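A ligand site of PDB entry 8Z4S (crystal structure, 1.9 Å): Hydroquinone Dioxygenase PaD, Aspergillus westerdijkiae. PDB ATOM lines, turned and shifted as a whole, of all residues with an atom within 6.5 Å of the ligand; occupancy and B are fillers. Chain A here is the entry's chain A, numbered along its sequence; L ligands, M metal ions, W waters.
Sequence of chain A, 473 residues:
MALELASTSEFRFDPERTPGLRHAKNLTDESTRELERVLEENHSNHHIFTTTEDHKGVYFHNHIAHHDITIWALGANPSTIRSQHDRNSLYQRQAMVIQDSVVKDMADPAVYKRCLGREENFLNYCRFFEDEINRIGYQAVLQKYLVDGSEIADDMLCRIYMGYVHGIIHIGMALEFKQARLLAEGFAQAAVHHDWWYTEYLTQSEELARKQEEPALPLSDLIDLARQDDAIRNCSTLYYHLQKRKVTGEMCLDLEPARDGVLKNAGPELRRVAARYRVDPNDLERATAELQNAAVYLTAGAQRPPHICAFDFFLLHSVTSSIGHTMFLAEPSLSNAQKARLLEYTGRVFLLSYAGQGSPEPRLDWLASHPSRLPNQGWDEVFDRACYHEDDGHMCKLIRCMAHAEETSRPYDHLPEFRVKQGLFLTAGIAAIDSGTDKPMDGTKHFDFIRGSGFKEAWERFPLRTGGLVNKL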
ATOM      1  N   THR A  50      -2.971  -2.200 -34.767  1.00  0.00           N
ATOM      2  CA  THR A  50      -2.016  -2.924 -33.882  1.00  0.00           C
ATOM      3  C   THR A  50      -2.417  -4.362 -33.585  1.00  0.00           C
ATOM      4  O   THR A  50      -1.575  -5.051 -32.949  1.00  0.00           O
ATOM      5  CB  THR A  50      -1.886  -2.256 -32.530  1.00  0.00           C
ATOM      6  OG1 THR A  50      -3.157  -2.294 -31.890  1.00  0.00           O
ATOM      7  CG2 THR A  50      -1.326  -0.840 -32.700  1.00  0.00           C
ATOM      8  N   VAL A  58     -12.276  -6.964 -32.726  1.00  0.00           N
ATOM      9  CA  VAL A  58     -12.306  -5.701 -33.496  1.00  0.00           C
ATOM     10  C   VAL A  58     -10.855  -5.232 -33.622  1.00  0.00           C
ATOM     11  O   VAL A  58     -10.016  -5.646 -32.819  1.00  0.00           O
ATOM     12  CB  VAL A  58     -13.209  -4.633 -32.850  1.00  0.00           C
ATOM     13  CG1 VAL A  58     -14.655  -5.073 -32.710  1.00  0.00           C
ATOM     14  CG2 VAL A  58     -12.665  -4.154 -31.507  1.00  0.00           C
ATOM     15  N   TYR A  59     -10.563  -4.411 -34.618  1.00  0.00           N
ATOM     16  CA  TYR A  59      -9.215  -3.786 -34.790  1.00  0.00           C
ATOM     17  C   TYR A  59      -8.962  -2.854 -33.612  1.00  0.00           C
ATOM     18  O   TYR A  59      -9.841  -2.025 -33.152  1.00  0.00           O
ATOM     19  CB  TYR A  59      -9.079  -3.064 -36.129  1.00  0.00           C
ATOM     20  CG  TYR A  59      -8.986  -3.900 -37.372  1.00  0.00           C
ATOM     21  CD1 TYR A  59      -7.912  -4.726 -37.646  1.00  0.00           C
ATOM     22  CD2 TYR A  59      -9.944  -3.767 -38.353  1.00  0.00           C
ATOM     23  CE1 TYR A  59      -7.829  -5.461 -38.821  1.00  0.00           C
ATOM     24  CE2 TYR A  59      -9.890  -4.484 -39.542  1.00  0.00           C
ATOM     25  CZ  TYR A  59      -8.823  -5.337 -39.774  1.00  0.00           C
ATOM     26  OH  TYR A  59      -8.798  -6.011 -40.941  1.00  0.00           O
ATOM     27  N   PHE A  60      -7.771  -2.994 -33.051  1.00  0.00           N
ATOM     28  CA  PHE A  60      -7.163  -1.946 -32.183  1.00  0.00           C
ATOM     29  C   PHE A  60      -6.351  -1.036 -33.098  1.00  0.00           C
ATOM     30  O   PHE A  60      -5.802  -1.554 -34.077  1.00  0.00           O
ATOM     31  CB  PHE A  60      -6.300  -2.569 -31.089  1.00  0.00           C
ATOM     32  CG  PHE A  60      -7.073  -3.207 -29.961  1.00  0.00           C
ATOM     33  CD1 PHE A  60      -8.437  -3.467 -30.067  1.00  0.00           C
ATOM     34  CD2 PHE A  60      -6.406  -3.577 -28.791  1.00  0.00           C
ATOM     35  CE1 PHE A  60      -9.148  -4.040 -29.007  1.00  0.00           C
ATOM     36  CE2 PHE A  60      -7.116  -4.144 -27.738  1.00  0.00           C
ATOM     37  CZ  PHE A  60      -8.478  -4.389 -27.858  1.00  0.00           C
ATOM     38  N   HIS A  61      -6.320   0.272 -32.822  1.00  0.00           N
ATOM     39  CA  HIS A  61      -5.680   1.264 -33.725  1.00  0.00           C
ATOM     40  C   HIS A  61      -4.310   1.693 -33.216  1.00  0.00           C
ATOM     41  O   HIS A  61      -4.136   1.855 -32.010  1.00  0.00           O
ATOM     42  CB  HIS A  61      -6.602   2.495 -33.904  1.00  0.00           C
ATOM     43  CG  HIS A  61      -7.928   2.138 -34.448  1.00  0.00           C
ATOM     44  ND1 HIS A  61      -8.906   1.569 -33.676  1.00  0.00           N
ATOM     45  CD2 HIS A  61      -8.465   2.294 -35.680  1.00  0.00           C
ATOM     46  CE1 HIS A  61      -9.962   1.349 -34.425  1.00  0.00           C
ATOM     47  NE2 HIS A  61      -9.695   1.721 -35.649  1.00  0.00           N
ATOM     48  N   ASN A  62      -3.432   1.996 -34.163  1.00  0.00           N
ATOM     49  CA  ASN A  62      -2.110   2.632 -33.922  1.00  0.00           C
ATOM     50  C   ASN A  62      -2.386   4.115 -33.606  1.00  0.00           C
ATOM     51  O   ASN A  62      -2.813   4.833 -34.515  1.00  0.00           O
ATOM     52  CB  ASN A  62      -1.231   2.416 -35.147  1.00  0.00           C
ATOM     53  CG  ASN A  62       0.130   3.073 -35.006  1.00  0.00           C
ATOM     54  OD1 ASN A  62       0.468   3.532 -33.938  1.00  0.00           O
ATOM     55  ND2 ASN A  62       0.923   3.034 -36.073  1.00  0.00           N
ATOM     56  N   HIS A  63      -2.130   4.531 -32.381  1.00  0.00           N
ATOM     57  CA  HIS A  63      -2.345   5.924 -31.891  1.00  0.00           C
ATOM     58  C   HIS A  63      -1.031   6.687 -31.893  1.00  0.00           C
ATOM     59  O   HIS A  63      -1.005   7.812 -31.346  1.00  0.00           O
ATOM     60  CB  HIS A  63      -2.907   5.930 -30.500  1.00  0.00           C
ATOM     61  CG  HIS A  63      -4.322   5.501 -30.511  1.00  0.00           C
ATOM     62  ND1 HIS A  63      -4.670   4.196 -30.791  1.00  0.00           N
ATOM     63  CD2 HIS A  63      -5.460   6.185 -30.328  1.00  0.00           C
ATOM     64  CE1 HIS A  63      -5.978   4.101 -30.729  1.00  0.00           C
ATOM     65  NE2 HIS A  63      -6.504   5.305 -30.497  1.00  0.00           N
ATOM     66  N   GLY A 163     -14.748   2.328 -36.786  1.00  0.00           N
ATOM     67  CA  GLY A 163     -13.591   2.019 -35.917  1.00  0.00           C
ATOM     68  C   GLY A 163     -13.450   3.096 -34.882  1.00  0.00           C
ATOM     69  O   GLY A 163     -12.323   3.516 -34.628  1.00  0.00           O
ATOM     70  N   TYR A 164     -14.576   3.518 -34.292  1.00  0.00           N
ATOM     71  CA  TYR A 164     -14.642   4.548 -33.235  1.00  0.00           C
ATOM     72  C   TYR A 164     -13.977   5.860 -33.727  1.00  0.00           C
ATOM     73  O   TYR A 164     -13.182   6.448 -32.969  1.00  0.00           O
ATOM     74  CB  TYR A 164     -14.088   3.992 -31.912  1.00  0.00           C
ATOM     75  CG  TYR A 164     -14.662   2.615 -31.638  1.00  0.00           C
ATOM     76  CD1 TYR A 164     -16.015   2.446 -31.389  1.00  0.00           C
ATOM     77  CD2 TYR A 164     -13.880   1.473 -31.744  1.00  0.00           C
ATOM     78  CE1 TYR A 164     -16.565   1.180 -31.213  1.00  0.00           C
ATOM     79  CE2 TYR A 164     -14.410   0.208 -31.564  1.00  0.00           C
ATOM     80  CZ  TYR A 164     -15.760   0.054 -31.286  1.00  0.00           C
ATOM     81  OH  TYR A 164     -16.258  -1.209 -31.113  1.00  0.00           O
ATOM     82  N   HIS A 166     -11.702   6.902 -35.779  1.00  0.00           N
ATOM     83  CA  HIS A 166     -10.234   7.147 -35.867  1.00  0.00           C
ATOM     84  C   HIS A 166      -9.897   7.867 -37.191  1.00  0.00           C
ATOM     85  O   HIS A 166      -8.921   8.661 -37.158  1.00  0.00           O
ATOM     86  CB  HIS A 166      -9.399   5.881 -35.511  1.00  0.00           C
ATOM     87  CG  HIS A 166      -9.390   5.618 -34.028  1.00  0.00           C
ATOM     88  ND1 HIS A 166     -10.318   4.784 -33.407  1.00  0.00           N
ATOM     89  CD2 HIS A 166      -8.597   6.079 -33.029  1.00  0.00           C
ATOM     90  CE1 HIS A 166     -10.117   4.796 -32.092  1.00  0.00           C
ATOM     91  NE2 HIS A 166      -9.080   5.609 -31.821  1.00  0.00           N
ATOM     92  N   MET A 251     -10.073 -11.392 -23.146  1.00  0.00           N
ATOM     93  CA  MET A 251     -10.994 -10.287 -23.488  1.00  0.00           C
ATOM     94  C   MET A 251     -11.214 -10.321 -24.996  1.00  0.00           C
ATOM     95  O   MET A 251     -10.267 -10.574 -25.757  1.00  0.00           O
ATOM     96  CB  MET A 251     -10.390  -8.942 -23.075  1.00  0.00           C
ATOM     97  CG  MET A 251     -11.152  -7.756 -23.610  1.00  0.00           C
ATOM     98  SD  MET A 251     -10.617  -7.241 -25.270  1.00  0.00           S
ATOM     99  CE  MET A 251     -11.309  -5.574 -25.315  1.00  0.00           C
ATOM    100  N   LEU A 253     -14.194  -8.464 -28.210  1.00  0.00           N
ATOM    101  CA  LEU A 253     -15.382  -7.665 -28.552  1.00  0.00           C
ATOM    102  C   LEU A 253     -16.018  -8.378 -29.730  1.00  0.00           C
ATOM    103  O   LEU A 253     -16.145  -7.790 -30.803  1.00  0.00           O
ATOM    104  CB  LEU A 253     -14.938  -6.234 -28.906  1.00  0.00           C
ATOM    105  CG  LEU A 253     -14.821  -5.288 -27.721  1.00  0.00           C
ATOM    106  CD1 LEU A 253     -13.982  -4.061 -28.088  1.00  0.00           C
ATOM    107  CD2 LEU A 253     -16.213  -4.851 -27.283  1.00  0.00           C
ATOM    108  N   PHE A 313     -13.596   5.177 -21.915  1.00  0.00           N
ATOM    109  CA  PHE A 313     -12.691   4.922 -23.062  1.00  0.00           C
ATOM    110  C   PHE A 313     -13.411   5.199 -24.386  1.00  0.00           C
ATOM    111  O   PHE A 313     -12.808   5.763 -25.317  1.00  0.00           O
ATOM    112  CB  PHE A 313     -12.179   3.478 -23.053  1.00  0.00           C
ATOM    113  CG  PHE A 313     -11.202   3.229 -24.155  1.00  0.00           C
ATOM    114  CD1 PHE A 313      -9.900   3.704 -24.060  1.00  0.00           C
ATOM    115  CD2 PHE A 313     -11.587   2.594 -25.331  1.00  0.00           C
ATOM    116  CE1 PHE A 313      -9.004   3.516 -25.087  1.00  0.00           C
ATOM    117  CE2 PHE A 313     -10.681   2.407 -26.356  1.00  0.00           C
ATOM    118  CZ  PHE A 313      -9.385   2.883 -26.233  1.00  0.00           C
ATOM    119  N   PHE A 314     -14.656   4.754 -24.513  1.00  0.00           N
ATOM    120  CA  PHE A 314     -15.443   4.895 -25.769  1.00  0.00           C
ATOM    121  C   PHE A 314     -16.003   6.320 -25.831  1.00  0.00           C
ATOM    122  O   PHE A 314     -15.910   6.922 -26.887  1.00  0.00           O
ATOM    123  CB  PHE A 314     -16.475   3.760 -25.916  1.00  0.00           C
ATOM    124  CG  PHE A 314     -15.812   2.442 -26.225  1.00  0.00           C
ATOM    125  CD1 PHE A 314     -15.414   2.139 -27.522  1.00  0.00           C
ATOM    126  CD2 PHE A 314     -15.449   1.568 -25.211  1.00  0.00           C
ATOM    127  CE1 PHE A 314     -14.697   0.988 -27.801  1.00  0.00           C
ATOM    128  CE2 PHE A 314     -14.760   0.400 -25.495  1.00  0.00           C
ATOM    129  CZ  PHE A 314     -14.404   0.095 -26.787  1.00  0.00           C
ATOM    130  N   HIS A 317     -13.737   9.409 -27.261  1.00  0.00           N
ATOM    131  CA  HIS A 317     -13.513   9.601 -28.707  1.00  0.00           C
ATOM    132  C   HIS A 317     -14.470  10.683 -29.259  1.00  0.00           C
ATOM    133  O   HIS A 317     -14.153  11.256 -30.295  1.00  0.00           O
ATOM    134  CB  HIS A 317     -13.630   8.286 -29.493  1.00  0.00           C
ATOM    135  CG  HIS A 317     -12.478   7.398 -29.200  1.00  0.00           C
ATOM    136  ND1 HIS A 317     -12.341   6.794 -27.972  1.00  0.00           N
ATOM    137  CD2 HIS A 317     -11.338   7.122 -29.898  1.00  0.00           C
ATOM    138  CE1 HIS A 317     -11.191   6.139 -27.930  1.00  0.00           C
ATOM    139  NE2 HIS A 317     -10.566   6.314 -29.094  1.00  0.00           N
ATOM    140  N   ASP A 392      -1.194   5.381 -24.517  1.00  0.00           N
ATOM    141  CA  ASP A 392      -1.027   5.392 -25.978  1.00  0.00           C
ATOM    142  C   ASP A 392      -1.490   6.737 -26.524  1.00  0.00           C
ATOM    143  O   ASP A 392      -1.542   6.856 -27.760  1.00  0.00           O
ATOM    144  CB  ASP A 392      -1.790   4.243 -26.617  1.00  0.00           C
ATOM    145  CG  ASP A 392      -3.280   4.266 -26.315  1.00  0.00           C
ATOM    146  OD1 ASP A 392      -3.704   5.093 -25.438  1.00  0.00           O
ATOM    147  OD2 ASP A 392      -3.983   3.392 -26.888  1.00  0.00           O
ATOM    148  N   HIS A 394      -4.489   8.539 -25.300  1.00  0.00           N
ATOM    149  CA  HIS A 394      -5.915   8.925 -25.071  1.00  0.00           C
ATOM    150  C   HIS A 394      -5.997  10.025 -24.004  1.00  0.00           C
ATOM    151  O   HIS A 394      -6.837  10.964 -24.145  1.00  0.00           O
ATOM    152  CB  HIS A 394      -6.778   7.688 -24.731  1.00  0.00           C
ATOM    153  CG  HIS A 394      -7.039   6.861 -25.949  1.00  0.00           C
ATOM    154  ND1 HIS A 394      -6.179   5.841 -26.359  1.00  0.00           N
ATOM    155  CD2 HIS A 394      -7.978   6.988 -26.919  1.00  0.00           C
ATOM    156  CE1 HIS A 394      -6.644   5.296 -27.475  1.00  0.00           C
ATOM    157  NE2 HIS A 394      -7.762   6.019 -27.881  1.00  0.00           N
ATOM    158  N   MET A 441      -1.473   1.261 -18.678  1.00  0.00           N
ATOM    159  CA  MET A 441      -1.658   0.225 -19.709  1.00  0.00           C
ATOM    160  C   MET A 441      -0.826  -1.021 -19.390  1.00  0.00           C
ATOM    161  O   MET A 441       0.072  -0.948 -18.526  1.00  0.00           O
ATOM    162  CB  MET A 441      -1.307   0.745 -21.083  1.00  0.00           C
ATOM    163  CG  MET A 441      -2.262   1.846 -21.505  1.00  0.00           C
ATOM    164  SD  MET A 441      -1.951   2.322 -23.112  1.00  0.00           S
ATOM    165  CE  MET A 441      -2.539   0.951 -24.121  1.00  0.00           C
ATOM    166  N   THR A 444      -1.541  -3.349 -24.956  1.00  0.00           N
ATOM    167  CA  THR A 444      -2.693  -2.619 -25.542  1.00  0.00           C
ATOM    168  C   THR A 444      -3.878  -2.521 -24.576  1.00  0.00           C
ATOM    169  O   THR A 444      -4.872  -1.853 -24.918  1.00  0.00           O
ATOM    170  CB  THR A 444      -3.136  -3.206 -26.891  1.00  0.00           C
ATOM    171  OG1 THR A 444      -3.395  -4.605 -26.744  1.00  0.00           O
ATOM    172  CG2 THR A 444      -2.130  -2.950 -27.990  1.00  0.00           C
ATOM    173  N   LYS A 445      -3.797  -3.073 -23.390  1.00  0.00           N
ATOM    174  CA  LYS A 445      -4.900  -3.020 -22.412  1.00  0.00           C
ATOM    175  C   LYS A 445      -4.839  -1.735 -21.593  1.00  0.00           C
ATOM    176  O   LYS A 445      -3.764  -1.442 -21.008  1.00  0.00           O
ATOM    177  CB  LYS A 445      -4.901  -4.222 -21.462  1.00  0.00           C
ATOM    178  CG  LYS A 445      -6.154  -4.287 -20.608  1.00  0.00           C
ATOM    179  CD  LYS A 445      -6.431  -5.613 -19.917  1.00  0.00           C
ATOM    180  CE  LYS A 445      -7.531  -5.437 -18.890  1.00  0.00           C
ATOM    181  NZ  LYS A 445      -7.596  -6.543 -17.912  1.00  0.00           N
ATOM    182  N   HIS A 446      -5.971  -1.046 -21.488  1.00  0.00           N
ATOM    183  CA  HIS A 446      -6.126   0.204 -20.708  1.00  0.00           C
ATOM    184  C   HIS A 446      -6.717  -0.141 -19.366  1.00  0.00           C
ATOM    185  O   HIS A 446      -7.644  -0.937 -19.338  1.00  0.00           O
ATOM    186  CB  HIS A 446      -7.039   1.197 -21.437  1.00  0.00           C
ATOM    187  CG  HIS A 446      -6.388   1.950 -22.557  1.00  0.00           C
ATOM    188  ND1 HIS A 446      -5.733   3.121 -22.332  1.00  0.00           N
ATOM    189  CD2 HIS A 446      -6.289   1.700 -23.861  1.00  0.00           C
ATOM    190  CE1 HIS A 446      -5.287   3.578 -23.461  1.00  0.00           C
ATOM    191  NE2 HIS A 446      -5.603   2.763 -24.423  1.00  0.00           N
ATOM    192  N   ARG A 451     -15.084   1.440 -18.700  1.00  0.00           N
ATOM    193  CA  ARG A 451     -15.783   0.922 -19.881  1.00  0.00           C
ATOM    194  C   ARG A 451     -17.203   0.607 -19.419  1.00  0.00           C
ATOM    195  O   ARG A 451     -17.371  -0.201 -18.477  1.00  0.00           O
ATOM    196  CB  ARG A 451     -15.009  -0.250 -20.465  1.00  0.00           C
ATOM    197  CG  ARG A 451     -13.690   0.145 -21.103  1.00  0.00           C
ATOM    198  CD  ARG A 451     -13.084  -0.926 -21.992  1.00  0.00           C
ATOM    199  NE  ARG A 451     -11.843  -0.391 -22.548  1.00  0.00           N
ATOM    200  CZ  ARG A 451     -11.232  -0.761 -23.668  1.00  0.00           C
ATOM    201  NH1 ARG A 451     -11.732  -1.708 -24.450  1.00  0.00           N
ATOM    202  NH2 ARG A 451     -10.093  -0.168 -24.001  1.00  0.00           N
HETATM  203  C1  LIG L   1     -10.580   0.481 -30.823  1.00  0.00           C
HETATM  204  C2  LIG L   1      -9.660   0.256 -29.782  1.00  0.00           C
HETATM  205  C3  LIG L   1      -9.939  -0.538 -28.661  1.00  0.00           C
HETATM  206  C4  LIG L   1     -11.211  -1.186 -28.457  1.00  0.00           C
HETATM  207  C5  LIG L   1      -8.911  -0.703 -27.715  1.00  0.00           C
HETATM  208  O1  LIG L   1      -9.228  -1.437 -26.625  1.00  0.00           O
HETATM  209  C6  LIG L   1      -7.635  -0.116 -27.822  1.00  0.00           C
HETATM  210  C7  LIG L   1      -6.607  -0.302 -26.868  1.00  0.00           C
HETATM  211  C8  LIG L   1      -7.328   0.637 -28.965  1.00  0.00           C
HETATM  212  C9  LIG L   1      -8.371   0.823 -29.894  1.00  0.00           C
HETATM  213  O2  LIG L   1      -8.188   1.542 -30.976  1.00  0.00           O
HETATM  214 FE    FE M   1      -8.556   5.937 -29.857  1.00  0.00          FE
HETATM  215  O   HOH W   1      -9.067   3.653 -29.457  1.00  0.00           O
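The backbone carbonyl oxygen of His 61 sits at hydrogen-bond distance from a ring nitrogen (ND1) of His 63.
O of Gly 163 lies close to NE2 of His 61 (3.3 Å).
The backbone carbonyl oxygen (O) of Phe 60 sits at hydrogen-bond distance from the backbone NH (N) of Thr 50 (3.0 Å).
A ring nitrogen (ND1) of His 166 sits at hydrogen-bond distance from the backbone carbonyl oxygen (O) of Tyr 164, 3.3 Å away.
OD2 of Asp 392 sits at hydrogen-bond distance from NE2 of His 446.
The backbone carbonyl oxygen (O) of Phe 313 is in hydrogen-bond range of a ring nitrogen (ND1) of His 317 (2.9 Å).
A ring nitrogen (ND1) of His 166 lies within hydrogen-bond range of the backbone carbonyl oxygen of Gly 163 (2.7 Å).
O of Tyr 59 touches C1 of the ligand, 3.5 Å away.
CZ of Phe 60 touches O1 of the ligand (3.3 Å).
CE1 of His 63 touches O2 of the ligand (3.4 Å).
Tyr 164 touches the ligand.
His 166 touches the ligand.
Phe 313 touches the ligand (CE2 to C3, 3.8 Å).
Phe 314 touches the ligand (CZ to C4, 3.8 Å).
O of Thr 444 touches C7 of the ligand, 3.0 Å away.
His 446 touches the ligand (CD2 to C7, 3.6 Å).
Hydrophobic or aromatic side chains within 4 Å of the ligand: Phe 60, His 61, His 63, Tyr 164, His 166, Phe 313, Phe 314 and His 446.
Within 4 Å of the ligand: Tyr 59, Phe 60, His 61, His 63, Tyr 164, His 166, Phe 313, Phe 314, Thr 444, His 446 and Arg 451.
The nearest printed residue that does not touch the ligand is Leu 253 (4.01 Å).
The backbone NH of His 61 lies within hydrogen-bond range of an oxygen (O2) of the ligand (2.9 Å).
O2 of the ligand lies within hydrogen-bond range of ND1 of His 61 (2.8 Å).
An oxygen (O1) of the ligand lies within hydrogen-bond range of the guanidinium group (NH2) of Arg 451, 3.0 Å away.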
